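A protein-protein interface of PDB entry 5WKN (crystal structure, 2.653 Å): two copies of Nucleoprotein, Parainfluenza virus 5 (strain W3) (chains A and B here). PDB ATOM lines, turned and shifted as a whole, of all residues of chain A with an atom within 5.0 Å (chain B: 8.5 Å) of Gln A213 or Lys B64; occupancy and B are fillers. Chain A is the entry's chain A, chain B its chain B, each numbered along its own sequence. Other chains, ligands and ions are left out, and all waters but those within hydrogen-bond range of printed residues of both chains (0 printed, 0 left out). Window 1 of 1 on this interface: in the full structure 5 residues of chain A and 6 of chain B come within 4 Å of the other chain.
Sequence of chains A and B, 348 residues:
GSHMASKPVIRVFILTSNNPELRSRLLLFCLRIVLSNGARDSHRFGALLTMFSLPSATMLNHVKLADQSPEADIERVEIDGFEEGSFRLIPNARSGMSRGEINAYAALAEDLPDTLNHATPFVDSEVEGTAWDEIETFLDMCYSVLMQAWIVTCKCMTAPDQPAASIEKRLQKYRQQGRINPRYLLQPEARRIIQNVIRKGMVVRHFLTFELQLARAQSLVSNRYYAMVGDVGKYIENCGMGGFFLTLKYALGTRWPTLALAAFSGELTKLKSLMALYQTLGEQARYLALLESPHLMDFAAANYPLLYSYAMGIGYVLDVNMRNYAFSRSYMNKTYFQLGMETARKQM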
ATOM      1  N   THR A 209      11.159 -33.172  25.565  1.00  0.00           N
ATOM      2  CA  THR A 209      10.279 -32.223  24.884  1.00  0.00           C
ATOM      3  C   THR A 209       8.892 -32.215  25.505  1.00  0.00           C
ATOM      4  O   THR A 209       8.282 -31.150  25.658  1.00  0.00           O
ATOM      5  CB  THR A 209      10.167 -32.544  23.394  1.00  0.00           C
ATOM      6  OG1 THR A 209       9.697 -33.890  23.233  1.00  0.00           O
ATOM      7  CG2 THR A 209      11.510 -32.351  22.686  1.00  0.00           C
ATOM      8  N   PHE A 210       8.367 -33.392  25.844  1.00  0.00           N
ATOM      9  CA  PHE A 210       7.056 -33.450  26.477  1.00  0.00           C
ATOM     10  C   PHE A 210       7.054 -32.707  27.807  1.00  0.00           C
ATOM     11  O   PHE A 210       6.071 -32.036  28.146  1.00  0.00           O
ATOM     12  CB  PHE A 210       6.633 -34.907  26.656  1.00  0.00           C
ATOM     13  CG  PHE A 210       5.933 -35.472  25.461  1.00  0.00           C
ATOM     14  CD1 PHE A 210       4.596 -35.193  25.232  1.00  0.00           C
ATOM     15  CD2 PHE A 210       6.617 -36.254  24.548  1.00  0.00           C
ATOM     16  CE1 PHE A 210       3.949 -35.699  24.124  1.00  0.00           C
ATOM     17  CE2 PHE A 210       5.980 -36.761  23.437  1.00  0.00           C
ATOM     18  CZ  PHE A 210       4.642 -36.486  23.225  1.00  0.00           C
ATOM     19  N   GLU A 211       8.147 -32.798  28.568  1.00  0.00           N
ATOM     20  CA  GLU A 211       8.207 -32.069  29.828  1.00  0.00           C
ATOM     21  C   GLU A 211       8.226 -30.566  29.587  1.00  0.00           C
ATOM     22  O   GLU A 211       7.600 -29.805  30.334  1.00  0.00           O
ATOM     23  CB  GLU A 211       9.430 -32.501  30.638  1.00  0.00           C
ATOM     24  CG  GLU A 211       9.401 -33.946  31.118  1.00  0.00           C
ATOM     25  CD  GLU A 211       8.761 -34.110  32.491  1.00  0.00           C
ATOM     26  OE1 GLU A 211       7.514 -34.136  32.565  1.00  0.00           O
ATOM     27  OE2 GLU A 211       9.510 -34.208  33.497  1.00  0.00           O
ATOM     28  N   LEU A 212       8.937 -30.117  28.550  1.00  0.00           N
ATOM     29  CA  LEU A 212       8.930 -28.695  28.216  1.00  0.00           C
ATOM     30  C   LEU A 212       7.562 -28.259  27.705  1.00  0.00           C
ATOM     31  O   LEU A 212       7.098 -27.158  28.018  1.00  0.00           O
ATOM     32  CB  LEU A 212      10.020 -28.396  27.186  1.00  0.00           C
ATOM     33  CG  LEU A 212      11.462 -28.617  27.641  1.00  0.00           C
ATOM     34  CD1 LEU A 212      12.426 -28.533  26.478  1.00  0.00           C
ATOM     35  CD2 LEU A 212      11.834 -27.616  28.698  1.00  0.00           C
ATOM     36  N   GLN A 213       6.897 -29.112  26.929  1.00  0.00           N
ATOM     37  CA  GLN A 213       5.566 -28.770  26.439  1.00  0.00           C
ATOM     38  C   GLN A 213       4.559 -28.667  27.576  1.00  0.00           C
ATOM     39  O   GLN A 213       3.672 -27.807  27.538  1.00  0.00           O
ATOM     40  CB  GLN A 213       5.103 -29.795  25.405  1.00  0.00           C
ATOM     41  CG  GLN A 213       5.751 -29.622  24.041  1.00  0.00           C
ATOM     42  CD  GLN A 213       5.291 -30.674  23.058  1.00  0.00           C
ATOM     43  OE1 GLN A 213       4.904 -31.777  23.450  1.00  0.00           O
ATOM     44  NE2 GLN A 213       5.318 -30.342  21.775  1.00  0.00           N
ATOM     45  N   LEU A 214       4.683 -29.524  28.595  1.00  0.00           N
ATOM     46  CA  LEU A 214       3.834 -29.407  29.775  1.00  0.00           C
ATOM     47  C   LEU A 214       4.317 -28.312  30.715  1.00  0.00           C
ATOM     48  O   LEU A 214       3.511 -27.740  31.452  1.00  0.00           O
ATOM     49  CB  LEU A 214       3.762 -30.749  30.520  1.00  0.00           C
ATOM     50  CG  LEU A 214       3.188 -30.768  31.942  1.00  0.00           C
ATOM     51  CD1 LEU A 214       1.726 -30.317  31.937  1.00  0.00           C
ATOM     52  CD2 LEU A 214       3.315 -32.152  32.520  1.00  0.00           C
ATOM     53  N   ALA A 215       5.616 -28.016  30.724  1.00  0.00           N
ATOM     54  CA  ALA A 215       6.103 -26.894  31.520  1.00  0.00           C
ATOM     55  C   ALA A 215       5.330 -25.622  31.183  1.00  0.00           C
ATOM     56  O   ALA A 215       4.690 -25.018  32.052  1.00  0.00           O
ATOM     57  CB  ALA A 215       7.608 -26.702  31.311  1.00  0.00           C
ATOM     58  N   ARG A 216       5.349 -25.215  29.919  1.00  0.00           N
ATOM     59  CA  ARG A 216       4.435 -24.161  29.516  1.00  0.00           C
ATOM     60  C   ARG A 216       3.008 -24.704  29.520  1.00  0.00           C
ATOM     61  O   ARG A 216       2.775 -25.906  29.673  1.00  0.00           O
ATOM     62  CB  ARG A 216       4.823 -23.592  28.148  1.00  0.00           C
ATOM     63  CG  ARG A 216       4.827 -24.599  27.019  1.00  0.00           C
ATOM     64  CD  ARG A 216       5.464 -24.031  25.750  1.00  0.00           C
ATOM     65  NE  ARG A 216       5.369 -24.987  24.650  1.00  0.00           N
ATOM     66  CZ  ARG A 216       4.495 -24.897  23.651  1.00  0.00           C
ATOM     67  NH1 ARG A 216       3.646 -23.876  23.602  1.00  0.00           N
ATOM     68  NH2 ARG A 216       4.476 -25.824  22.701  1.00  0.00           N
ATOM     69  N   ALA A 217       2.041 -23.800  29.374  1.00  0.00           N
ATOM     70  CA  ALA A 217       0.629 -24.120  29.578  1.00  0.00           C
ATOM     71  C   ALA A 217       0.344 -24.533  31.021  1.00  0.00           C
ATOM     72  O   ALA A 217      -0.578 -25.314  31.276  1.00  0.00           O
ATOM     73  CB  ALA A 217       0.139 -25.202  28.602  1.00  0.00           C
ATOM     74  N   GLU A 283       4.188 -27.940  16.444  1.00  0.00           N
ATOM     75  CA  GLU A 283       4.708 -27.977  17.807  1.00  0.00           C
ATOM     76  C   GLU A 283       6.194 -28.312  17.834  1.00  0.00           C
ATOM     77  O   GLU A 283       6.935 -27.797  18.677  1.00  0.00           O
ATOM     78  CB  GLU A 283       3.916 -28.983  18.638  1.00  0.00           C
ATOM     79  CG  GLU A 283       2.698 -28.388  19.313  1.00  0.00           C
ATOM     80  CD  GLU A 283       3.039 -27.723  20.633  1.00  0.00           C
ATOM     81  OE1 GLU A 283       3.297 -28.455  21.617  1.00  0.00           O
ATOM     82  OE2 GLU A 283       3.058 -26.474  20.688  1.00  0.00           O
ATOM     83  N   GLN A 284       6.651 -29.160  16.914  1.00  0.00           N
ATOM     84  CA  GLN A 284       8.056 -29.543  16.887  1.00  0.00           C
ATOM     85  C   GLN A 284       8.972 -28.433  16.377  1.00  0.00           C
ATOM     86  O   GLN A 284      10.194 -28.603  16.436  1.00  0.00           O
ATOM     87  CB  GLN A 284       8.232 -30.798  16.028  1.00  0.00           C
ATOM     88  CG  GLN A 284       7.116 -31.822  16.189  1.00  0.00           C
ATOM     89  CD  GLN A 284       7.403 -32.840  17.283  1.00  0.00           C
ATOM     90  OE1 GLN A 284       8.353 -33.619  17.190  1.00  0.00           O
ATOM     91  NE2 GLN A 284       6.578 -32.834  18.329  1.00  0.00           N
ATOM     92  N   TYR A 287      11.497 -27.013  18.874  1.00  0.00           N
ATOM     93  CA  TYR A 287      12.362 -28.001  19.515  1.00  0.00           C
ATOM     94  C   TYR A 287      13.273 -28.723  18.525  1.00  0.00           C
ATOM     95  O   TYR A 287      13.669 -29.865  18.764  1.00  0.00           O
ATOM     96  CB  TYR A 287      11.533 -29.025  20.290  1.00  0.00           C
ATOM     97  CG  TYR A 287      10.620 -28.437  21.340  1.00  0.00           C
ATOM     98  CD1 TYR A 287      11.134 -27.758  22.436  1.00  0.00           C
ATOM     99  CD2 TYR A 287       9.240 -28.585  21.246  1.00  0.00           C
ATOM    100  CE1 TYR A 287      10.295 -27.229  23.401  1.00  0.00           C
ATOM    101  CE2 TYR A 287       8.392 -28.061  22.202  1.00  0.00           C
ATOM    102  CZ  TYR A 287       8.925 -27.384  23.280  1.00  0.00           C
ATOM    103  OH  TYR A 287       8.090 -26.856  24.241  1.00  0.00           O
ATOM    104  N   VAL B  12     -13.958 -21.743  24.294  1.00  0.00           N
ATOM    105  CA  VAL B  12     -13.916 -22.655  25.430  1.00  0.00           C
ATOM    106  C   VAL B  12     -13.856 -21.818  26.709  1.00  0.00           C
ATOM    107  O   VAL B  12     -12.788 -21.306  27.064  1.00  0.00           O
ATOM    108  CB  VAL B  12     -12.717 -23.611  25.341  1.00  0.00           C
ATOM    109  CG1 VAL B  12     -12.617 -24.467  26.590  1.00  0.00           C
ATOM    110  CG2 VAL B  12     -12.811 -24.490  24.099  1.00  0.00           C
ATOM    111  N   THR B  58      -6.100 -32.375  32.306  1.00  0.00           N
ATOM    112  CA  THR B  58      -5.224 -32.573  31.157  1.00  0.00           C
ATOM    113  C   THR B  58      -5.747 -31.837  29.930  1.00  0.00           C
ATOM    114  O   THR B  58      -5.013 -31.066  29.302  1.00  0.00           O
ATOM    115  CB  THR B  58      -5.076 -34.072  30.891  1.00  0.00           C
ATOM    116  OG1 THR B  58      -4.113 -34.615  31.801  1.00  0.00           O
ATOM    117  CG2 THR B  58      -4.645 -34.355  29.461  1.00  0.00           C
ATOM    118  N   MET B  59      -7.019 -32.052  29.575  1.00  0.00           N
ATOM    119  CA  MET B  59      -7.594 -31.332  28.442  1.00  0.00           C
ATOM    120  C   MET B  59      -7.543 -29.823  28.657  1.00  0.00           C
ATOM    121  O   MET B  59      -7.420 -29.059  27.695  1.00  0.00           O
ATOM    122  CB  MET B  59      -9.033 -31.789  28.204  1.00  0.00           C
ATOM    123  CG  MET B  59      -9.736 -31.067  27.071  1.00  0.00           C
ATOM    124  SD  MET B  59     -11.455 -31.566  26.902  1.00  0.00           S
ATOM    125  CE  MET B  59     -11.272 -33.174  26.142  1.00  0.00           C
ATOM    126  N   LEU B  60      -7.631 -29.384  29.913  1.00  0.00           N
ATOM    127  CA  LEU B  60      -7.514 -27.963  30.222  1.00  0.00           C
ATOM    128  C   LEU B  60      -6.146 -27.421  29.830  1.00  0.00           C
ATOM    129  O   LEU B  60      -6.033 -26.293  29.342  1.00  0.00           O
ATOM    130  CB  LEU B  60      -7.779 -27.746  31.709  1.00  0.00           C
ATOM    131  CG  LEU B  60      -9.197 -27.271  32.000  1.00  0.00           C
ATOM    132  CD1 LEU B  60      -9.595 -27.529  33.450  1.00  0.00           C
ATOM    133  CD2 LEU B  60      -9.251 -25.804  31.678  1.00  0.00           C
ATOM    134  N   ASN B  61      -5.089 -28.208  30.037  1.00  0.00           N
ATOM    135  CA  ASN B  61      -3.763 -27.795  29.598  1.00  0.00           C
ATOM    136  C   ASN B  61      -3.562 -27.987  28.101  1.00  0.00           C
ATOM    137  O   ASN B  61      -2.669 -27.362  27.518  1.00  0.00           O
ATOM    138  CB  ASN B  61      -2.690 -28.561  30.379  1.00  0.00           C
ATOM    139  CG  ASN B  61      -2.785 -28.326  31.873  1.00  0.00           C
ATOM    140  OD1 ASN B  61      -3.372 -27.337  32.322  1.00  0.00           O
ATOM    141  ND2 ASN B  61      -2.213 -29.237  32.653  1.00  0.00           N
ATOM    142  N   HIS B  62      -4.375 -28.830  27.464  1.00  0.00           N
ATOM    143  CA  HIS B  62      -4.243 -29.033  26.028  1.00  0.00           C
ATOM    144  C   HIS B  62      -4.834 -27.867  25.246  1.00  0.00           C
ATOM    145  O   HIS B  62      -4.282 -27.473  24.213  1.00  0.00           O
ATOM    146  CB  HIS B  62      -4.902 -30.351  25.621  1.00  0.00           C
ATOM    147  CG  HIS B  62      -4.023 -31.552  25.803  1.00  0.00           C
ATOM    148  ND1 HIS B  62      -4.405 -32.652  26.544  1.00  0.00           N
ATOM    149  CD2 HIS B  62      -2.781 -31.826  25.337  1.00  0.00           C
ATOM    150  CE1 HIS B  62      -3.435 -33.549  26.527  1.00  0.00           C
ATOM    151  NE2 HIS B  62      -2.438 -33.072  25.804  1.00  0.00           N
ATOM    152  N   VAL B  63      -5.940 -27.293  25.720  1.00  0.00           N
ATOM    153  CA  VAL B  63      -6.546 -26.157  25.031  1.00  0.00           C
ATOM    154  C   VAL B  63      -5.652 -24.934  25.216  1.00  0.00           C
ATOM    155  O   VAL B  63      -5.723 -24.236  26.233  1.00  0.00           O
ATOM    156  CB  VAL B  63      -7.987 -25.891  25.514  1.00  0.00           C
ATOM    157  CG1 VAL B  63      -8.942 -26.868  24.862  1.00  0.00           C
ATOM    158  CG2 VAL B  63      -8.095 -26.002  27.018  1.00  0.00           C
ATOM    159  N   LYS B  64      -4.788 -24.677  24.238  1.00  0.00           N
ATOM    160  CA  LYS B  64      -3.852 -23.565  24.299  1.00  0.00           C
ATOM    161  C   LYS B  64      -4.029 -22.679  23.073  1.00  0.00           C
ATOM    162  O   LYS B  64      -4.066 -23.172  21.938  1.00  0.00           O
ATOM    163  CB  LYS B  64      -2.409 -24.063  24.397  1.00  0.00           C
ATOM    164  CG  LYS B  64      -2.039 -25.098  23.346  1.00  0.00           C
ATOM    165  CD  LYS B  64      -0.662 -25.670  23.616  1.00  0.00           C
ATOM    166  CE  LYS B  64      -0.626 -26.385  24.957  1.00  0.00           C
ATOM    167  NZ  LYS B  64       0.747 -26.844  25.303  1.00  0.00           N
ATOM    168  N   LEU B  65      -4.141 -21.372  23.310  1.00  0.00           N
ATOM    169  CA  LEU B  65      -4.228 -20.397  22.234  1.00  0.00           C
ATOM    170  C   LEU B  65      -2.874 -20.045  21.636  1.00  0.00           C
ATOM    171  O   LEU B  65      -2.837 -19.395  20.586  1.00  0.00           O
ATOM    172  CB  LEU B  65      -4.877 -19.096  22.717  1.00  0.00           C
ATOM    173  CG  LEU B  65      -6.306 -19.041  23.253  1.00  0.00           C
ATOM    174  CD1 LEU B  65      -6.321 -19.529  24.670  1.00  0.00           C
ATOM    175  CD2 LEU B  65      -6.836 -17.612  23.180  1.00  0.00           C
ATOM    176  N   ALA B  66      -1.773 -20.455  22.270  1.00  0.00           N
ATOM    177  CA  ALA B  66      -0.472 -19.867  21.963  1.00  0.00           C
ATOM    178  C   ALA B  66      -0.087 -20.065  20.500  1.00  0.00           C
ATOM    179  O   ALA B  66       0.264 -19.105  19.806  1.00  0.00           O
ATOM    180  CB  ALA B  66       0.596 -20.454  22.887  1.00  0.00           C
ATOM    181  N   ASP B  67      -0.150 -21.299  20.011  1.00  0.00           N
ATOM    182  CA  ASP B  67       0.432 -21.648  18.714  1.00  0.00           C
ATOM    183  C   ASP B  67      -0.659 -21.684  17.651  1.00  0.00           C
ATOM    184  O   ASP B  67      -1.262 -22.726  17.391  1.00  0.00           O
ATOM    185  CB  ASP B  67       1.165 -22.982  18.800  1.00  0.00           C
ATOM    186  CG  ASP B  67       2.665 -22.812  18.955  1.00  0.00           C
ATOM    187  OD1 ASP B  67       3.101 -21.730  19.410  1.00  0.00           O
ATOM    188  OD2 ASP B  67       3.408 -23.760  18.617  1.00  0.00           O
ATOM    189  N   GLN B  68      -0.891 -20.533  17.011  1.00  0.00           N
ATOM    190  CA  GLN B  68      -1.813 -20.426  15.880  1.00  0.00           C
ATOM    191  C   GLN B  68      -3.179 -21.013  16.248  1.00  0.00           C
ATOM    192  O   GLN B  68      -3.631 -22.029  15.719  1.00  0.00           O
ATOM    193  CB  GLN B  68      -1.203 -21.094  14.638  1.00  0.00           C
ATOM    194  CG  GLN B  68      -2.078 -21.146  13.392  1.00  0.00           C
ATOM    195  CD  GLN B  68      -2.609 -22.547  13.138  1.00  0.00           C
ATOM    196  OE1 GLN B  68      -1.854 -23.519  13.144  1.00  0.00           O
ATOM    197  NE2 GLN B  68      -3.920 -22.659  12.947  1.00  0.00           N
ATOM    198  N   SER B  69      -3.818 -20.366  17.204  1.00  0.00           N
ATOM    199  CA  SER B  69      -5.049 -20.908  17.752  1.00  0.00           C
ATOM    200  C   SER B  69      -6.217 -20.673  16.804  1.00  0.00           C
ATOM    201  O   SER B  69      -6.400 -19.550  16.320  1.00  0.00           O
ATOM    202  CB  SER B  69      -5.362 -20.273  19.095  1.00  0.00           C
ATOM    203  OG  SER B  69      -5.366 -18.855  19.012  1.00  0.00           O
ATOM    204  N   PRO B  70      -6.999 -21.709  16.484  1.00  0.00           N
ATOM    205  CA  PRO B  70      -8.428 -21.515  16.231  1.00  0.00           C
ATOM    206  C   PRO B  70      -9.229 -21.547  17.522  1.00  0.00           C
ATOM    207  O   PRO B  70     -10.422 -21.213  17.514  1.00  0.00           O
ATOM    208  CB  PRO B  70      -8.777 -22.707  15.331  1.00  0.00           C
ATOM    209  CG  PRO B  70      -7.840 -23.788  15.793  1.00  0.00           C
ATOM    210  CD  PRO B  70      -6.578 -23.107  16.271  1.00  0.00           C
ATOM    211  N   GLU B  71      -8.587 -21.940  18.620  1.00  0.00           N
ATOM    212  CA  GLU B  71      -9.193 -22.004  19.939  1.00  0.00           C
ATOM    213  C   GLU B  71      -9.038 -20.674  20.661  1.00  0.00           C
ATOM    214  O   GLU B  71      -8.036 -19.975  20.510  1.00  0.00           O
ATOM    215  CB  GLU B  71      -8.544 -23.105  20.778  1.00  0.00           C
ATOM    216  CG  GLU B  71      -8.613 -24.478  20.166  1.00  0.00           C
ATOM    217  CD  GLU B  71      -9.868 -25.215  20.569  1.00  0.00           C
ATOM    218  OE1 GLU B  71     -10.955 -24.846  20.079  1.00  0.00           O
ATOM    219  OE2 GLU B  71      -9.772 -26.159  21.384  1.00  0.00           O
ATOM    220  N   ALA B  72     -10.035 -20.340  21.471  1.00  0.00           N
ATOM    221  CA  ALA B  72      -9.964 -19.161  22.320  1.00  0.00           C
ATOM    222  C   ALA B  72     -10.466 -19.540  23.702  1.00  0.00           C
ATOM    223  O   ALA B  72     -11.621 -19.950  23.850  1.00  0.00           O
ATOM    224  CB  ALA B  72     -10.783 -18.007  21.736  1.00  0.00           C
ATOM    225  N   ASP B  73      -9.595 -19.421  24.707  1.00  0.00           N
ATOM    226  CA  ASP B  73     -10.024 -19.659  26.079  1.00  0.00           C
ATOM    227  C   ASP B  73     -11.112 -18.693  26.515  1.00  0.00           C
ATOM    228  O   ASP B  73     -11.721 -18.905  27.569  1.00  0.00           O
ATOM    229  CB  ASP B  73      -8.846 -19.529  27.049  1.00  0.00           C
ATOM    230  CG  ASP B  73      -8.025 -20.801  27.162  1.00  0.00           C
ATOM    231  OD1 ASP B  73      -8.222 -21.713  26.335  1.00  0.00           O
ATOM    232  OD2 ASP B  73      -7.163 -20.877  28.068  1.00  0.00           O
ATOM    233  N   PHE B 207      -9.476 -33.770  20.724  1.00  0.00           N
ATOM    234  CA  PHE B 207      -9.224 -33.677  22.156  1.00  0.00           C
ATOM    235  C   PHE B 207      -9.703 -34.917  22.901  1.00  0.00           C
ATOM    236  O   PHE B 207      -9.117 -35.286  23.927  1.00  0.00           O
ATOM    237  CB  PHE B 207      -9.887 -32.423  22.727  1.00  0.00           C
ATOM    238  CG  PHE B 207      -9.232 -31.141  22.288  1.00  0.00           C
ATOM    239  CD1 PHE B 207      -7.999 -30.763  22.800  1.00  0.00           C
ATOM    240  CD2 PHE B 207      -9.844 -30.317  21.362  1.00  0.00           C
ATOM    241  CE1 PHE B 207      -7.394 -29.586  22.393  1.00  0.00           C
ATOM    242  CE2 PHE B 207      -9.242 -29.147  20.948  1.00  0.00           C
ATOM    243  CZ  PHE B 207      -8.019 -28.778  21.466  1.00  0.00           C
ATOM    244  N   PHE B 210      -6.926 -37.458  23.508  1.00  0.00           N
ATOM    245  CA  PHE B 210      -6.069 -37.213  24.664  1.00  0.00           C
ATOM    246  C   PHE B 210      -6.702 -37.731  25.950  1.00  0.00           C
ATOM    247  O   PHE B 210      -5.987 -38.187  26.847  1.00  0.00           O
ATOM    248  CB  PHE B 210      -5.745 -35.724  24.778  1.00  0.00           C
ATOM    249  CG  PHE B 210      -4.810 -35.240  23.717  1.00  0.00           C
ATOM    250  CD1 PHE B 210      -3.529 -35.759  23.624  1.00  0.00           C
ATOM    251  CD2 PHE B 210      -5.209 -34.279  22.801  1.00  0.00           C
ATOM    252  CE1 PHE B 210      -2.658 -35.329  22.636  1.00  0.00           C
ATOM    253  CE2 PHE B 210      -4.341 -33.842  21.809  1.00  0.00           C
ATOM    254  CZ  PHE B 210      -3.065 -34.370  21.728  1.00  0.00           C
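The side-chain carboxylate (OE2) of Glu A283 lies close to the side-chain carboxylate (OD2) of Asp B67.
NE2 of Gln A213 is in hydrogen-bond range of OE1 of Glu A283 (2.8 Å).
The guanidinium group of Arg A216 lies within salt-bridge range of the side-chain carboxylate of Glu A283 (2.5 Å).
Gln A213 touches Lys B64 (O to NZ, 3.8 Å).
O of Ala A217 touches OD1 of Asn B61 (3.6 Å).
Ala A217 touches Lys B64 (CB to NZ, 3.7 Å).
Of the printed residues of chain B, Gln A213 touches Lys B64.
Leu A214 touches none of the printed residues of chain B.
Printed residues of chain B within 4 Å of Ala A217: Asn B61 (3.6 Å) and Lys B64 (3.7 Å).
Of the printed residues of chain A, Asn B61 touches Ala A217 (3.6 Å).
Of the printed residues of chain A, Lys B64 touches Gln A213 (3.8 Å) and Ala A217 (3.7 Å).
The nearest residue of chain B that does not touch Gln A213 is Asn B61 (6.4 Å).
The nearest residue of chain A that does not touch Lys B64 is Arg A216 (4.5 Å).
The nearest printed residue of chain B that does not touch Glu A283 is Lys B64 (4.8 Å).
Printed residues of chain B that touch a printed residue of chain A: Asn B61, Lys B64 and Asp B67.
Printed residues of chain A that touch a printed residue of chain B: Gln A213, Ala A217 and Glu A283.
Hydrophobic or aromatic side chains of chain A that line the printed part of chain B: Ala A217.
Position printed for both chains: 210.
Of the 4 pairs that touch across the chains among the printed residues, none has its exchanged pair printed and touching as well.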
